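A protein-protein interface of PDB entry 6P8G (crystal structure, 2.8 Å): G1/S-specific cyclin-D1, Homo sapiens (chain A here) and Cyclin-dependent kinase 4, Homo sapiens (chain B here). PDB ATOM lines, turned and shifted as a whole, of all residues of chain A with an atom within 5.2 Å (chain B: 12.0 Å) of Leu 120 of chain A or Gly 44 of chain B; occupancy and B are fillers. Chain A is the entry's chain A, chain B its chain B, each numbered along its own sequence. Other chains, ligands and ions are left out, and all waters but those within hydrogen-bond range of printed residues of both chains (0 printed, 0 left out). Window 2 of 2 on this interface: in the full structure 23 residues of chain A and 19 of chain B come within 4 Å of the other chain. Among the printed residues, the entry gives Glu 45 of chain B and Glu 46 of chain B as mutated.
Among the printed residues, merely in contact across the chains: Phe 90 of chain A with Glu 46 of chain B, Glu 123 of chain A with Gly 47 of chain B, Leu 120 of chain A with Gly 47 of chain B, Leu 124 of chain A with Ile 86 of chain B, Leu 120 of chain A with Gly 44 of chain B, Leu 124 of chain A with Ser 80 of chain B and Leu 120 of chain A with Glu 46 of chain B.
The backbone carbonyl oxygen of Glu 85 of chain B lies close to the side-chain hydroxyl of Ser 80 of chain B, at 3.3 Å.
Of the 11 printed residues of chain A, 5 touch a printed residue of chain B.
Printed residues of chain A that touch a printed residue of chain B: Phe 90, Ala 103, Leu 120, Glu 123 and Leu 124.
Hydrophobic or aromatic side chains of chain A within 4 Å of the printed part of chain B: Phe 90, Ala 103, Leu 120 and Leu 124.
Among the printed residues, no Asp or Glu carboxylate lies within 4 Å of a Lys or Arg side-chain nitrogen of the other chain.
The side-chain carboxylate (OE2) of Glu 123 of chain A sits at hydrogen-bond distance from the backbone NH (N) of Leu 48 of chain B (2.9 Å).
The backbone NH (N) of Ala 103 of chain A sits close to the side-chain carboxylate (OE1) of Glu 46 of chain B, at 2.4 Å.
Leu 120 of chain A touches three residues of chain B.
Gly 44 of chain B touches just one residue of chain A: Leu 120 (3.8 Å).
Printed residues of chain B within 4 Å of Ala 103 of chain A: Glu 46 (2.4 Å).
No residue of chain B comes within 4 Å of Pro 116 of chain A.
No residue of chain B comes within 4 Å of Leu 119 of chain A.
Of chain B, only Gly 47 and Leu 48 come within 4 Å of Glu 123 of chain A.
Of chain B, only Ser 80 (3.8 Å) and Ile 86 (3.6 Å) come within 4 Å of Leu 124 of chain A.
Of the printed residues of chain A, Ile 86 of chain B touches Leu 124.
Of the printed residues of chain A, Gly 47 of chain B touches Leu 120 and Glu 123.
Printed residues of chain A within 4 Å of Glu 46 of chain B: Phe 90 (3.1 Å), Ala 103 (2.4 Å) and Leu 120 (3.8 Å).
The nearest printed residue of chain A that does not touch Ser 80 of chain B is Gln 121 of chain A (6.3 Å).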
ATOM      1  N   PHE A  90     -13.065 -24.268 -29.769  1.00  0.00           N
ATOM      2  CA  PHE A  90     -13.149 -22.900 -30.270  1.00  0.00           C
ATOM      3  C   PHE A  90     -11.942 -22.077 -29.838  1.00  0.00           C
ATOM      4  O   PHE A  90     -11.438 -21.252 -30.609  1.00  0.00           O
ATOM      5  CB  PHE A  90     -14.449 -22.260 -29.785  1.00  0.00           C
ATOM      6  CG  PHE A  90     -14.761 -20.941 -30.429  1.00  0.00           C
ATOM      7  CD1 PHE A  90     -14.930 -20.846 -31.798  1.00  0.00           C
ATOM      8  CD2 PHE A  90     -14.905 -19.797 -29.658  1.00  0.00           C
ATOM      9  CE1 PHE A  90     -15.226 -19.634 -32.391  1.00  0.00           C
ATOM     10  CE2 PHE A  90     -15.201 -18.583 -30.245  1.00  0.00           C
ATOM     11  CZ  PHE A  90     -15.362 -18.501 -31.613  1.00  0.00           C
ATOM     12  N   ALA A 103     -17.674 -20.062 -34.874  1.00  0.00           N
ATOM     13  CA  ALA A 103     -18.607 -20.462 -33.825  1.00  0.00           C
ATOM     14  C   ALA A 103     -19.846 -21.128 -34.405  1.00  0.00           C
ATOM     15  O   ALA A 103     -20.440 -22.002 -33.764  1.00  0.00           O
ATOM     16  CB  ALA A 103     -19.005 -19.248 -32.986  1.00  0.00           C
ATOM     17  N   PRO A 116     -24.822 -19.949 -30.997  1.00  0.00           N
ATOM     18  CA  PRO A 116     -23.530 -19.247 -31.130  1.00  0.00           C
ATOM     19  C   PRO A 116     -23.161 -18.375 -29.939  1.00  0.00           C
ATOM     20  O   PRO A 116     -22.024 -18.451 -29.456  1.00  0.00           O
ATOM     21  CB  PRO A 116     -23.725 -18.427 -32.411  1.00  0.00           C
ATOM     22  CG  PRO A 116     -24.690 -19.232 -33.211  1.00  0.00           C
ATOM     23  CD  PRO A 116     -25.648 -19.817 -32.211  1.00  0.00           C
ATOM     24  N   GLU A 117     -24.084 -17.542 -29.449  1.00  0.00           N
ATOM     25  CA  GLU A 117     -23.750 -16.681 -28.317  1.00  0.00           C
ATOM     26  C   GLU A 117     -23.524 -17.492 -27.046  1.00  0.00           C
ATOM     27  O   GLU A 117     -22.692 -17.114 -26.212  1.00  0.00           O
ATOM     28  CB  GLU A 117     -24.842 -15.628 -28.107  1.00  0.00           C
ATOM     29  CG  GLU A 117     -24.811 -14.948 -26.739  1.00  0.00           C
ATOM     30  CD  GLU A 117     -24.185 -13.562 -26.773  1.00  0.00           C
ATOM     31  OE1 GLU A 117     -24.455 -12.764 -25.850  1.00  0.00           O
ATOM     32  OE2 GLU A 117     -23.420 -13.272 -27.717  1.00  0.00           O
ATOM     33  N   GLU A 118     -24.234 -18.612 -26.885  1.00  0.00           N
ATOM     34  CA  GLU A 118     -23.966 -19.495 -25.755  1.00  0.00           C
ATOM     35  C   GLU A 118     -22.542 -20.027 -25.793  1.00  0.00           C
ATOM     36  O   GLU A 118     -21.934 -20.257 -24.740  1.00  0.00           O
ATOM     37  CB  GLU A 118     -24.961 -20.655 -25.741  1.00  0.00           C
ATOM     38  CG  GLU A 118     -26.411 -20.229 -25.843  1.00  0.00           C
ATOM     39  CD  GLU A 118     -27.367 -21.353 -25.502  1.00  0.00           C
ATOM     40  OE1 GLU A 118     -28.457 -21.065 -24.965  1.00  0.00           O
ATOM     41  OE2 GLU A 118     -27.024 -22.524 -25.770  1.00  0.00           O
ATOM     42  N   LEU A 119     -21.994 -20.231 -26.991  1.00  0.00           N
ATOM     43  CA  LEU A 119     -20.597 -20.635 -27.106  1.00  0.00           C
ATOM     44  C   LEU A 119     -19.665 -19.468 -26.813  1.00  0.00           C
ATOM     45  O   LEU A 119     -18.613 -19.649 -26.188  1.00  0.00           O
ATOM     46  CB  LEU A 119     -20.330 -21.202 -28.501  1.00  0.00           C
ATOM     47  CG  LEU A 119     -18.923 -21.735 -28.767  1.00  0.00           C
ATOM     48  CD1 LEU A 119     -18.970 -23.213 -29.123  1.00  0.00           C
ATOM     49  CD2 LEU A 119     -18.255 -20.938 -29.872  1.00  0.00           C
ATOM     50  N   LEU A 120     -20.033 -18.262 -27.253  1.00  0.00           N
ATOM     51  CA  LEU A 120     -19.201 -17.094 -26.986  1.00  0.00           C
ATOM     52  C   LEU A 120     -19.189 -16.755 -25.501  1.00  0.00           C
ATOM     53  O   LEU A 120     -18.152 -16.356 -24.958  1.00  0.00           O
ATOM     54  CB  LEU A 120     -19.686 -15.901 -27.809  1.00  0.00           C
ATOM     55  CG  LEU A 120     -19.658 -16.077 -29.330  1.00  0.00           C
ATOM     56  CD1 LEU A 120     -19.798 -14.736 -30.030  1.00  0.00           C
ATOM     57  CD2 LEU A 120     -18.386 -16.784 -29.771  1.00  0.00           C
ATOM     58  N   GLN A 121     -20.331 -16.907 -24.826  1.00  0.00           N
ATOM     59  CA  GLN A 121     -20.367 -16.691 -23.384  1.00  0.00           C
ATOM     60  C   GLN A 121     -19.595 -17.779 -22.649  1.00  0.00           C
ATOM     61  O   GLN A 121     -18.942 -17.507 -21.635  1.00  0.00           O
ATOM     62  CB  GLN A 121     -21.813 -16.630 -22.894  1.00  0.00           C
ATOM     63  CG  GLN A 121     -22.329 -15.219 -22.667  1.00  0.00           C
ATOM     64  CD  GLN A 121     -23.842 -15.138 -22.709  1.00  0.00           C
ATOM     65  OE1 GLN A 121     -24.532 -16.157 -22.662  1.00  0.00           O
ATOM     66  NE2 GLN A 121     -24.367 -13.921 -22.801  1.00  0.00           N
ATOM     67  N   MET A 122     -19.659 -19.017 -23.147  1.00  0.00           N
ATOM     68  CA  MET A 122     -18.869 -20.088 -22.550  1.00  0.00           C
ATOM     69  C   MET A 122     -17.380 -19.890 -22.805  1.00  0.00           C
ATOM     70  O   MET A 122     -16.550 -20.363 -22.021  1.00  0.00           O
ATOM     71  CB  MET A 122     -19.329 -21.444 -23.088  1.00  0.00           C
ATOM     72  CG  MET A 122     -18.727 -22.639 -22.365  1.00  0.00           C
ATOM     73  SD  MET A 122     -19.232 -22.735 -20.639  1.00  0.00           S
ATOM     74  CE  MET A 122     -17.963 -23.806 -19.970  1.00  0.00           C
ATOM     75  N   GLU A 123     -17.024 -19.197 -23.890  1.00  0.00           N
ATOM     76  CA  GLU A 123     -15.620 -18.882 -24.134  1.00  0.00           C
ATOM     77  C   GLU A 123     -15.069 -17.981 -23.038  1.00  0.00           C
ATOM     78  O   GLU A 123     -13.991 -18.238 -22.491  1.00  0.00           O
ATOM     79  CB  GLU A 123     -15.457 -18.225 -25.506  1.00  0.00           C
ATOM     80  CG  GLU A 123     -14.031 -17.783 -25.805  1.00  0.00           C
ATOM     81  CD  GLU A 123     -13.947 -16.803 -26.959  1.00  0.00           C
ATOM     82  OE1 GLU A 123     -13.194 -17.075 -27.916  1.00  0.00           O
ATOM     83  OE2 GLU A 123     -14.632 -15.760 -26.904  1.00  0.00           O
ATOM     84  N   LEU A 124     -15.806 -16.921 -22.698  1.00  0.00           N
ATOM     85  CA  LEU A 124     -15.369 -16.027 -21.632  1.00  0.00           C
ATOM     86  C   LEU A 124     -15.288 -16.748 -20.295  1.00  0.00           C
ATOM     87  O   LEU A 124     -14.406 -16.451 -19.480  1.00  0.00           O
ATOM     88  CB  LEU A 124     -16.313 -14.828 -21.530  1.00  0.00           C
ATOM     89  CG  LEU A 124     -15.930 -13.563 -22.302  1.00  0.00           C
ATOM     90  CD1 LEU A 124     -15.763 -13.849 -23.789  1.00  0.00           C
ATOM     91  CD2 LEU A 124     -16.973 -12.486 -22.078  1.00  0.00           C
ATOM     92  N   ARG B  40      -9.835  -2.360 -24.496  1.00  0.00           N
ATOM     93  CA  ARG B  40     -11.113  -2.744 -25.078  1.00  0.00           C
ATOM     94  C   ARG B  40     -10.868  -3.365 -26.446  1.00  0.00           C
ATOM     95  O   ARG B  40     -10.197  -2.768 -27.293  1.00  0.00           O
ATOM     96  CB  ARG B  40     -12.042  -1.535 -25.197  1.00  0.00           C
ATOM     97  N   VAL B  41     -11.401  -4.565 -26.656  1.00  0.00           N
ATOM     98  CA  VAL B  41     -11.173  -5.291 -27.902  1.00  0.00           C
ATOM     99  C   VAL B  41     -12.484  -5.357 -28.683  1.00  0.00           C
ATOM    100  O   VAL B  41     -13.563  -5.251 -28.082  1.00  0.00           O
ATOM    101  CB  VAL B  41     -10.579  -6.684 -27.627  1.00  0.00           C
ATOM    102  CG1 VAL B  41      -9.495  -6.596 -26.559  1.00  0.00           C
ATOM    103  CG2 VAL B  41     -11.652  -7.665 -27.219  1.00  0.00           C
ATOM    104  N   PRO B  42     -12.435  -5.512 -30.025  1.00  0.00           N
ATOM    105  CA  PRO B  42     -13.651  -5.399 -30.851  1.00  0.00           C
ATOM    106  C   PRO B  42     -14.856  -6.210 -30.385  1.00  0.00           C
ATOM    107  O   PRO B  42     -15.879  -5.613 -30.029  1.00  0.00           O
ATOM    108  CB  PRO B  42     -13.167  -5.882 -32.222  1.00  0.00           C
ATOM    109  CG  PRO B  42     -11.739  -5.472 -32.262  1.00  0.00           C
ATOM    110  CD  PRO B  42     -11.218  -5.611 -30.853  1.00  0.00           C
ATOM    111  N   ASN B  43     -14.770  -7.548 -30.425  1.00  0.00           N
ATOM    112  CA  ASN B  43     -15.813  -8.451 -29.932  1.00  0.00           C
ATOM    113  C   ASN B  43     -17.024  -8.474 -30.858  1.00  0.00           C
ATOM    114  O   ASN B  43     -17.391  -7.462 -31.463  1.00  0.00           O
ATOM    115  CB  ASN B  43     -16.207  -8.074 -28.494  1.00  0.00           C
ATOM    116  CG  ASN B  43     -17.618  -8.529 -28.082  1.00  0.00           C
ATOM    117  OD1 ASN B  43     -18.195  -9.464 -28.629  1.00  0.00           O
ATOM    118  ND2 ASN B  43     -18.174  -7.835 -27.091  1.00  0.00           N
ATOM    119  N   GLY B  44     -17.644  -9.648 -30.966  1.00  0.00           N
ATOM    120  CA  GLY B  44     -18.889  -9.810 -31.686  1.00  0.00           C
ATOM    121  C   GLY B  44     -18.848 -10.960 -32.668  1.00  0.00           C
ATOM    122  O   GLY B  44     -19.600 -11.932 -32.539  1.00  0.00           O
ATOM    123  N   GLU B  45     -17.944 -10.854 -33.642  1.00  0.00           N
ATOM    124  CA  GLU B  45     -17.874 -11.798 -34.753  1.00  0.00           C
ATOM    125  C   GLU B  45     -17.784 -13.244 -34.268  1.00  0.00           C
ATOM    126  O   GLU B  45     -18.688 -14.051 -34.506  1.00  0.00           O
ATOM    127  CB  GLU B  45     -16.690 -11.416 -35.663  1.00  0.00           C
ATOM    128  CG  GLU B  45     -15.254 -11.514 -35.076  1.00  0.00           C
ATOM    129  CD  GLU B  45     -15.016 -10.690 -33.809  1.00  0.00           C
ATOM    130  OE1 GLU B  45     -13.947 -10.865 -33.186  1.00  0.00           O
ATOM    131  OE2 GLU B  45     -15.880  -9.868 -33.434  1.00  0.00           O
ATOM    132  N   GLU B  46     -16.703 -13.585 -33.573  1.00  0.00           N
ATOM    133  CA  GLU B  46     -16.451 -14.953 -33.138  1.00  0.00           C
ATOM    134  C   GLU B  46     -15.769 -14.920 -31.772  1.00  0.00           C
ATOM    135  O   GLU B  46     -14.690 -15.478 -31.576  1.00  0.00           O
ATOM    136  CB  GLU B  46     -15.601 -15.712 -34.160  1.00  0.00           C
ATOM    137  CG  GLU B  46     -16.097 -15.657 -35.600  1.00  0.00           C
ATOM    138  CD  GLU B  46     -17.164 -16.693 -35.891  1.00  0.00           C
ATOM    139  OE1 GLU B  46     -17.168 -17.743 -35.216  1.00  0.00           O
ATOM    140  OE2 GLU B  46     -17.996 -16.458 -36.793  1.00  0.00           O
ATOM    141  N   GLY B  47     -16.391 -14.241 -30.812  1.00  0.00           N
ATOM    142  CA  GLY B  47     -15.802 -14.151 -29.493  1.00  0.00           C
ATOM    143  C   GLY B  47     -14.576 -13.254 -29.469  1.00  0.00           C
ATOM    144  O   GLY B  47     -14.492 -12.239 -30.170  1.00  0.00           O
ATOM    145  N   LEU B  48     -13.601 -13.645 -28.648  1.00  0.00           N
ATOM    146  CA  LEU B  48     -12.403 -12.844 -28.472  1.00  0.00           C
ATOM    147  C   LEU B  48     -11.531 -12.896 -29.725  1.00  0.00           C
ATOM    148  O   LEU B  48     -11.486 -13.915 -30.420  1.00  0.00           O
ATOM    149  CB  LEU B  48     -11.609 -13.333 -27.266  1.00  0.00           C
ATOM    150  CG  LEU B  48     -12.358 -13.360 -25.933  1.00  0.00           C
ATOM    151  CD1 LEU B  48     -11.846 -14.491 -25.056  1.00  0.00           C
ATOM    152  CD2 LEU B  48     -12.228 -12.022 -25.220  1.00  0.00           C
ATOM    153  N   PRO B  49     -10.833 -11.805 -30.040  1.00  0.00           N
ATOM    154  CA  PRO B  49      -9.959 -11.802 -31.217  1.00  0.00           C
ATOM    155  C   PRO B  49      -8.813 -12.791 -31.065  1.00  0.00           C
ATOM    156  O   PRO B  49      -8.425 -13.174 -29.959  1.00  0.00           O
ATOM    157  CB  PRO B  49      -9.443 -10.357 -31.278  1.00  0.00           C
ATOM    158  CG  PRO B  49     -10.405  -9.565 -30.448  1.00  0.00           C
ATOM    159  CD  PRO B  49     -10.866 -10.494 -29.372  1.00  0.00           C
ATOM    160  N   ILE B  50      -8.271 -13.208 -32.211  1.00  0.00           N
ATOM    161  CA  ILE B  50      -7.150 -14.145 -32.204  1.00  0.00           C
ATOM    162  C   ILE B  50      -5.939 -13.519 -31.530  1.00  0.00           C
ATOM    163  O   ILE B  50      -5.261 -14.160 -30.719  1.00  0.00           O
ATOM    164  CB  ILE B  50      -6.823 -14.602 -33.638  1.00  0.00           C
ATOM    165  CG1 ILE B  50      -8.075 -15.137 -34.331  1.00  0.00           C
ATOM    166  CG2 ILE B  50      -5.729 -15.656 -33.623  1.00  0.00           C
ATOM    167  CD1 ILE B  50      -7.900 -15.333 -35.819  1.00  0.00           C
ATOM    168  N   THR B  52      -5.889 -11.267 -29.274  1.00  0.00           N
ATOM    169  CA  THR B  52      -6.099 -11.040 -27.848  1.00  0.00           C
ATOM    170  C   THR B  52      -5.806 -12.297 -27.039  1.00  0.00           C
ATOM    171  O   THR B  52      -5.096 -12.243 -26.028  1.00  0.00           O
ATOM    172  CB  THR B  52      -7.528 -10.557 -27.597  1.00  0.00           C
ATOM    173  OG1 THR B  52      -7.754  -9.336 -28.311  1.00  0.00           O
ATOM    174  CG2 THR B  52      -7.755 -10.318 -26.111  1.00  0.00           C
ATOM    175  N   VAL B  53      -6.338 -13.443 -27.471  1.00  0.00           N
ATOM    176  CA  VAL B  53      -6.181 -14.663 -26.683  1.00  0.00           C
ATOM    177  C   VAL B  53      -4.748 -15.174 -26.736  1.00  0.00           C
ATOM    178  O   VAL B  53      -4.289 -15.843 -25.802  1.00  0.00           O
ATOM    179  CB  VAL B  53      -7.176 -15.741 -27.153  1.00  0.00           C
ATOM    180  CG1 VAL B  53      -8.600 -15.329 -26.826  1.00  0.00           C
ATOM    181  CG2 VAL B  53      -7.017 -16.006 -28.641  1.00  0.00           C
ATOM    182  N   ALA B  78     -11.411 -10.212 -17.675  1.00  0.00           N
ATOM    183  CA  ALA B  78     -12.290  -9.835 -18.773  1.00  0.00           C
ATOM    184  C   ALA B  78     -13.684  -9.545 -18.232  1.00  0.00           C
ATOM    185  O   ALA B  78     -14.143 -10.196 -17.289  1.00  0.00           O
ATOM    186  CB  ALA B  78     -12.356 -10.940 -19.828  1.00  0.00           C
ATOM    187  N   THR B  79     -14.357  -8.564 -18.834  1.00  0.00           N
ATOM    188  CA  THR B  79     -15.658  -8.110 -18.348  1.00  0.00           C
ATOM    189  C   THR B  79     -16.537  -7.741 -19.534  1.00  0.00           C
ATOM    190  O   THR B  79     -16.240  -6.784 -20.256  1.00  0.00           O
ATOM    191  CB  THR B  79     -15.508  -6.921 -17.403  1.00  0.00           C
ATOM    192  OG1 THR B  79     -14.622  -7.269 -16.331  1.00  0.00           O
ATOM    193  CG2 THR B  79     -16.855  -6.544 -16.833  1.00  0.00           C
ATOM    194  N   SER B  80     -17.619  -8.489 -19.727  1.00  0.00           N
ATOM    195  CA  SER B  80     -18.543  -8.237 -20.827  1.00  0.00           C
ATOM    196  C   SER B  80     -19.614  -7.225 -20.430  1.00  0.00           C
ATOM    197  O   SER B  80     -20.444  -6.830 -21.251  1.00  0.00           O
ATOM    198  CB  SER B  80     -19.198  -9.540 -21.288  1.00  0.00           C
ATOM    199  OG  SER B  80     -19.978  -9.332 -22.454  1.00  0.00           O
ATOM    200  N   ARG B  84     -22.110  -7.134 -27.504  1.00  0.00           N
ATOM    201  CA  ARG B  84     -22.194  -5.902 -26.730  1.00  0.00           C
ATOM    202  C   ARG B  84     -20.827  -5.238 -26.608  1.00  0.00           C
ATOM    203  O   ARG B  84     -20.387  -4.529 -27.512  1.00  0.00           O
ATOM    204  CB  ARG B  84     -22.773  -6.177 -25.342  1.00  0.00           C
ATOM    205  N   GLU B  85     -20.158  -5.475 -25.482  1.00  0.00           N
ATOM    206  CA  GLU B  85     -18.849  -4.894 -25.228  1.00  0.00           C
ATOM    207  C   GLU B  85     -18.066  -5.826 -24.315  1.00  0.00           C
ATOM    208  O   GLU B  85     -18.640  -6.512 -23.467  1.00  0.00           O
ATOM    209  CB  GLU B  85     -18.969  -3.496 -24.603  1.00  0.00           C
ATOM    210  CG  GLU B  85     -17.649  -2.859 -24.176  1.00  0.00           C
ATOM    211  CD  GLU B  85     -16.867  -2.277 -25.340  1.00  0.00           C
ATOM    212  OE1 GLU B  85     -16.637  -1.049 -25.343  1.00  0.00           O
ATOM    213  OE2 GLU B  85     -16.476  -3.043 -26.246  1.00  0.00           O
ATOM    214  N   ILE B  86     -16.749  -5.857 -24.511  1.00  0.00           N
ATOM    215  CA  ILE B  86     -15.839  -6.602 -23.649  1.00  0.00           C
ATOM    216  C   ILE B  86     -14.624  -5.727 -23.376  1.00  0.00           C
ATOM    217  O   ILE B  86     -14.181  -4.968 -24.246  1.00  0.00           O
ATOM    218  CB  ILE B  86     -15.424  -7.949 -24.278  1.00  0.00           C
ATOM    219  CG1 ILE B  86     -14.530  -8.749 -23.332  1.00  0.00           C
ATOM    220  CG2 ILE B  86     -14.674  -7.719 -25.550  1.00  0.00           C
ATOM    221  CD1 ILE B  86     -15.252  -9.340 -22.163  1.00  0.00           C
ATOM    222  N   LYS B  87     -14.097  -5.819 -22.159  1.00  0.00           N
ATOM    223  CA  LYS B  87     -12.915  -5.056 -21.776  1.00  0.00           C
ATOM    224  C   LYS B  87     -12.102  -5.914 -20.821  1.00  0.00           C
ATOM    225  O   LYS B  87     -12.530  -6.157 -19.687  1.00  0.00           O
ATOM    226  CB  LYS B  87     -13.298  -3.725 -21.134  1.00  0.00           C
